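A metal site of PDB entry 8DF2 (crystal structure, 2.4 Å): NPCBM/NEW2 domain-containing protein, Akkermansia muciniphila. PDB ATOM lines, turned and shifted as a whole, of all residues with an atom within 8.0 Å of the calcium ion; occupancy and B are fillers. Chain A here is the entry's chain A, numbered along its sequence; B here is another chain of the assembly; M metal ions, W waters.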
ATOM      1  N   LEU A 338     -19.269  -5.095 -11.367  1.00  0.00           N
ATOM      2  CA  LEU A 338     -19.902  -4.900 -12.661  1.00  0.00           C
ATOM      3  C   LEU A 338     -19.153  -5.764 -13.678  1.00  0.00           C
ATOM      4  O   LEU A 338     -17.922  -5.737 -13.740  1.00  0.00           O
ATOM      5  CB  LEU A 338     -19.873  -3.431 -13.083  1.00  0.00           C
ATOM      6  CG  LEU A 338     -20.796  -2.471 -12.328  1.00  0.00           C
ATOM      7  CD1 LEU A 338     -20.691  -1.081 -12.927  1.00  0.00           C
ATOM      8  CD2 LEU A 338     -22.217  -2.961 -12.393  1.00  0.00           C
ATOM      9  N   ASP A 339     -19.898  -6.566 -14.445  1.00  0.00           N
ATOM     10  CA  ASP A 339     -19.303  -7.585 -15.309  1.00  0.00           C
ATOM     11  C   ASP A 339     -20.029  -7.613 -16.649  1.00  0.00           C
ATOM     12  O   ASP A 339     -21.138  -8.166 -16.739  1.00  0.00           O
ATOM     13  CB  ASP A 339     -19.329  -8.951 -14.629  1.00  0.00           C
ATOM     14  CG  ASP A 339     -18.336  -9.918 -15.218  1.00  0.00           C
ATOM     15  OD1 ASP A 339     -17.785  -9.625 -16.308  1.00  0.00           O
ATOM     16  OD2 ASP A 339     -18.118 -10.987 -14.590  1.00  0.00           O
ATOM     17  N   PRO A 340     -19.428  -7.055 -17.705  1.00  0.00           N
ATOM     18  CA  PRO A 340     -20.060  -7.139 -19.020  1.00  0.00           C
ATOM     19  C   PRO A 340     -20.121  -8.577 -19.501  1.00  0.00           C
ATOM     20  O   PRO A 340     -19.218  -9.381 -19.200  1.00  0.00           O
ATOM     21  CB  PRO A 340     -19.129  -6.287 -19.913  1.00  0.00           C
ATOM     22  CG  PRO A 340     -18.293  -5.464 -18.950  1.00  0.00           C
ATOM     23  CD  PRO A 340     -18.177  -6.288 -17.705  1.00  0.00           C
ATOM     24  N   PRO A 341     -21.157  -8.955 -20.260  1.00  0.00           N
ATOM     25  CA  PRO A 341     -21.241 -10.347 -20.727  1.00  0.00           C
ATOM     26  C   PRO A 341     -20.061 -10.700 -21.621  1.00  0.00           C
ATOM     27  O   PRO A 341     -19.512  -9.848 -22.329  1.00  0.00           O
ATOM     28  CB  PRO A 341     -22.570 -10.379 -21.510  1.00  0.00           C
ATOM     29  CG  PRO A 341     -22.865  -8.978 -21.827  1.00  0.00           C
ATOM     30  CD  PRO A 341     -22.308  -8.161 -20.702  1.00  0.00           C
ATOM     31  N   GLY A 342     -19.660 -11.965 -21.546  1.00  0.00           N
ATOM     32  CA  GLY A 342     -18.514 -12.443 -22.281  1.00  0.00           C
ATOM     33  C   GLY A 342     -17.203 -12.141 -21.566  1.00  0.00           C
ATOM     34  O   GLY A 342     -17.111 -11.284 -20.682  1.00  0.00           O
ATOM     35  N   GLY A 343     -16.165 -12.889 -21.960  1.00  0.00           N
ATOM     36  CA  GLY A 343     -14.841 -12.684 -21.423  1.00  0.00           C
ATOM     37  C   GLY A 343     -14.656 -13.105 -19.984  1.00  0.00           C
ATOM     38  O   GLY A 343     -13.713 -12.644 -19.332  1.00  0.00           O
ATOM     39  N   SER A 344     -15.539 -13.956 -19.464  1.00  0.00           N
ATOM     40  CA  SER A 344     -15.470 -14.398 -18.066  1.00  0.00           C
ATOM     41  C   SER A 344     -15.540 -13.186 -17.143  1.00  0.00           C
ATOM     42  O   SER A 344     -16.077 -12.141 -17.521  1.00  0.00           O
ATOM     43  CB  SER A 344     -14.195 -15.217 -17.817  1.00  0.00           C
ATOM     44  OG  SER A 344     -14.041 -15.511 -16.447  1.00  0.00           O
ATOM     45  N   ASP A 345     -15.010 -13.300 -15.921  1.00  0.00           N
ATOM     46  CA  ASP A 345     -15.018 -12.167 -14.991  1.00  0.00           C
ATOM     47  C   ASP A 345     -13.718 -11.370 -15.011  1.00  0.00           C
ATOM     48  O   ASP A 345     -13.506 -10.531 -14.129  1.00  0.00           O
ATOM     49  CB  ASP A 345     -15.330 -12.648 -13.557  1.00  0.00           C
ATOM     50  CG  ASP A 345     -14.435 -13.798 -13.088  1.00  0.00           C
ATOM     51  OD1 ASP A 345     -13.750 -14.420 -13.931  1.00  0.00           O
ATOM     52  OD2 ASP A 345     -14.408 -14.060 -11.866  1.00  0.00           O
ATOM     53  N   TYR A 346     -12.872 -11.595 -16.021  1.00  0.00           N
ATOM     54  CA  TYR A 346     -11.615 -10.849 -16.134  1.00  0.00           C
ATOM     55  C   TYR A 346     -11.876  -9.367 -16.364  1.00  0.00           C
ATOM     56  O   TYR A 346     -11.127  -8.511 -15.878  1.00  0.00           O
ATOM     57  CB  TYR A 346     -10.772 -11.413 -17.263  1.00  0.00           C
ATOM     58  CG  TYR A 346     -10.157 -12.754 -16.984  1.00  0.00           C
ATOM     59  CD1 TYR A 346      -9.160 -12.894 -16.024  1.00  0.00           C
ATOM     60  CD2 TYR A 346     -10.560 -13.878 -17.692  1.00  0.00           C
ATOM     61  CE1 TYR A 346      -8.586 -14.121 -15.766  1.00  0.00           C
ATOM     62  CE2 TYR A 346      -9.988 -15.108 -17.444  1.00  0.00           C
ATOM     63  CZ  TYR A 346      -9.002 -15.230 -16.485  1.00  0.00           C
ATOM     64  OH  TYR A 346      -8.428 -16.457 -16.227  1.00  0.00           O
ATOM     65  N   ASP A 347     -12.917  -9.041 -17.120  1.00  0.00           N
ATOM     66  CA  ASP A 347     -13.211  -7.666 -17.472  1.00  0.00           C
ATOM     67  C   ASP A 347     -14.154  -7.003 -16.473  1.00  0.00           C
ATOM     68  O   ASP A 347     -14.680  -5.915 -16.758  1.00  0.00           O
ATOM     69  CB  ASP A 347     -13.793  -7.597 -18.894  1.00  0.00           C
ATOM     70  CG  ASP A 347     -15.055  -8.425 -19.044  1.00  0.00           C
ATOM     71  OD1 ASP A 347     -15.320  -9.264 -18.162  1.00  0.00           O
ATOM     72  OD2 ASP A 347     -15.784  -8.223 -20.042  1.00  0.00           O
ATOM     73  N   SER A 348     -14.350  -7.608 -15.309  1.00  0.00           N
ATOM     74  CA  SER A 348     -15.196  -7.000 -14.307  1.00  0.00           C
ATOM     75  C   SER A 348     -14.433  -5.902 -13.571  1.00  0.00           C
ATOM     76  O   SER A 348     -13.208  -5.859 -13.562  1.00  0.00           O
ATOM     77  CB  SER A 348     -15.689  -8.033 -13.299  1.00  0.00           C
ATOM     78  OG  SER A 348     -14.678  -8.368 -12.353  1.00  0.00           O
ATOM     79  N   ARG A 367     -18.764   2.657 -14.903  1.00  0.00           N
ATOM     80  CA  ARG A 367     -18.117   2.070 -16.065  1.00  0.00           C
ATOM     81  C   ARG A 367     -18.127   3.125 -17.153  1.00  0.00           C
ATOM     82  O   ARG A 367     -18.965   3.097 -18.063  1.00  0.00           O
ATOM     83  CB  ARG A 367     -18.813   0.785 -16.512  1.00  0.00           C
ATOM     84  CG  ARG A 367     -17.985  -0.054 -17.448  1.00  0.00           C
ATOM     85  CD  ARG A 367     -17.285  -1.156 -16.712  1.00  0.00           C
ATOM     86  NE  ARG A 367     -16.482  -1.972 -17.615  1.00  0.00           N
ATOM     87  CZ  ARG A 367     -15.810  -3.052 -17.261  1.00  0.00           C
ATOM     88  NH1 ARG A 367     -15.812  -3.497 -16.016  1.00  0.00           N
ATOM     89  NH2 ARG A 367     -15.112  -3.710 -18.183  1.00  0.00           N
ATOM     90  N   TYR A 370     -19.027   3.051 -21.242  1.00  0.00           N
ATOM     91  CA  TYR A 370     -19.550   1.726 -21.560  1.00  0.00           C
ATOM     92  C   TYR A 370     -20.680   1.844 -22.579  1.00  0.00           C
ATOM     93  O   TYR A 370     -21.607   2.640 -22.394  1.00  0.00           O
ATOM     94  CB  TYR A 370     -20.046   1.034 -20.292  1.00  0.00           C
ATOM     95  CG  TYR A 370     -20.477  -0.411 -20.503  1.00  0.00           C
ATOM     96  CD1 TYR A 370     -19.552  -1.375 -20.887  1.00  0.00           C
ATOM     97  CD2 TYR A 370     -21.800  -0.805 -20.299  1.00  0.00           C
ATOM     98  CE1 TYR A 370     -19.927  -2.697 -21.081  1.00  0.00           C
ATOM     99  CE2 TYR A 370     -22.189  -2.124 -20.491  1.00  0.00           C
ATOM    100  CZ  TYR A 370     -21.244  -3.065 -20.885  1.00  0.00           C
ATOM    101  OH  TYR A 370     -21.612  -4.382 -21.083  1.00  0.00           O
ATOM    102  N   ILE A 375     -25.390  -5.118 -18.384  1.00  0.00           N
ATOM    103  CA  ILE A 375     -24.226  -5.465 -17.566  1.00  0.00           C
ATOM    104  C   ILE A 375     -24.716  -6.179 -16.315  1.00  0.00           C
ATOM    105  O   ILE A 375     -25.776  -5.859 -15.759  1.00  0.00           O
ATOM    106  CB  ILE A 375     -23.380  -4.215 -17.230  1.00  0.00           C
ATOM    107  CG1 ILE A 375     -22.016  -4.604 -16.660  1.00  0.00           C
ATOM    108  CG2 ILE A 375     -24.108  -3.274 -16.292  1.00  0.00           C
ATOM    109  CD1 ILE A 375     -20.979  -3.509 -16.762  1.00  0.00           C
ATOM    110  N   GLU A 376     -23.952  -7.179 -15.886  1.00  0.00           N
ATOM    111  CA  GLU A 376     -24.283  -7.953 -14.698  1.00  0.00           C
ATOM    112  C   GLU A 376     -23.699  -7.275 -13.468  1.00  0.00           C
ATOM    113  O   GLU A 376     -22.570  -6.806 -13.487  1.00  0.00           O
ATOM    114  CB  GLU A 376     -23.748  -9.381 -14.813  1.00  0.00           C
ATOM    115  CG  GLU A 376     -23.805 -10.192 -13.520  1.00  0.00           C
ATOM    116  CD  GLU A 376     -23.672 -11.693 -13.765  1.00  0.00           C
ATOM    117  OE1 GLU A 376     -24.415 -12.216 -14.628  1.00  0.00           O
ATOM    118  OE2 GLU A 376     -22.825 -12.336 -13.111  1.00  0.00           O
ATOM    119  N   ARG A 378     -22.954  -8.133  -9.516  1.00  0.00           N
ATOM    120  CA  ARG A 378     -22.876  -9.056  -8.395  1.00  0.00           C
ATOM    121  C   ARG A 378     -22.700  -8.253  -7.102  1.00  0.00           C
ATOM    122  O   ARG A 378     -21.921  -7.299  -7.074  1.00  0.00           O
ATOM    123  CB  ARG A 378     -21.721 -10.039  -8.572  1.00  0.00           C
ATOM    124  CG  ARG A 378     -21.939 -11.076  -9.676  1.00  0.00           C
ATOM    125  CD  ARG A 378     -20.815 -12.108  -9.695  1.00  0.00           C
ATOM    126  NE  ARG A 378     -19.539 -11.542 -10.126  1.00  0.00           N
ATOM    127  CZ  ARG A 378     -19.216 -11.273 -11.389  1.00  0.00           C
ATOM    128  NH1 ARG A 378     -20.072 -11.490 -12.382  1.00  0.00           N
ATOM    129  NH2 ARG A 378     -18.012 -10.773 -11.668  1.00  0.00           N
ATOM    130  N   GLN B 132     -19.947  -6.216 -26.959  1.00  0.00           N
ATOM    131  CA  GLN B 132     -21.125  -6.738 -26.277  1.00  0.00           C
ATOM    132  C   GLN B 132     -22.420  -6.328 -26.953  1.00  0.00           C
ATOM    133  O   GLN B 132     -23.404  -7.071 -26.894  1.00  0.00           O
ATOM    134  CB  GLN B 132     -21.134  -6.276 -24.817  1.00  0.00           C
ATOM    135  CG  GLN B 132     -20.003  -6.832 -23.968  1.00  0.00           C
ATOM    136  CD  GLN B 132     -18.796  -5.896 -23.918  1.00  0.00           C
ATOM    137  OE1 GLN B 132     -18.895  -4.717 -24.264  1.00  0.00           O
ATOM    138  NE2 GLN B 132     -17.663  -6.414 -23.472  1.00  0.00           N
HETATM  139 CA    CA M   1     -17.447 -10.567 -18.385  1.00  0.00          CA
HETATM  140  O   HOH W   1     -19.272 -12.607 -18.067  1.00  0.00           O
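OD2 of Asp 339 is in salt-bridge range of NH2 of Arg 378, at 2.9 Å.
The backbone NH (N) of Asp 339 lies within hydrogen-bond range of the backbone carbonyl oxygen (O) of Glu 376, 2.8 Å away.
The backbone carbonyl oxygen (O) of Asp 347 sits at hydrogen-bond distance from the guanidinium group (NH2) of Arg 367 (2.7 Å).
The side-chain hydroxyl (OG) of Ser 344 lies within hydrogen-bond range of the side-chain carboxylate (OD1) of Asp 345 (2.8 Å).
The nearest printed residue that does not touch the calcium ion is Gly 343 (4.1 Å).
The backbone carbonyl oxygen (O) of Ser 344 binds the calcium ion, 2.3 Å away.
The calcium ion is bound by the backbone carbonyl oxygen (O) of Pro 340 (2.3 Å).
The calcium ion is bound by OD1 of Asp 339, 2.3 Å away.
O of Gly 342 binds the calcium ion (2.4 Å).
OD1 of Asp 347 binds the calcium ion, 2.5 Å away.
Water W1 binds the calcium ion (2.8 Å).
The calcium ion has six donor atoms within binding distance.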
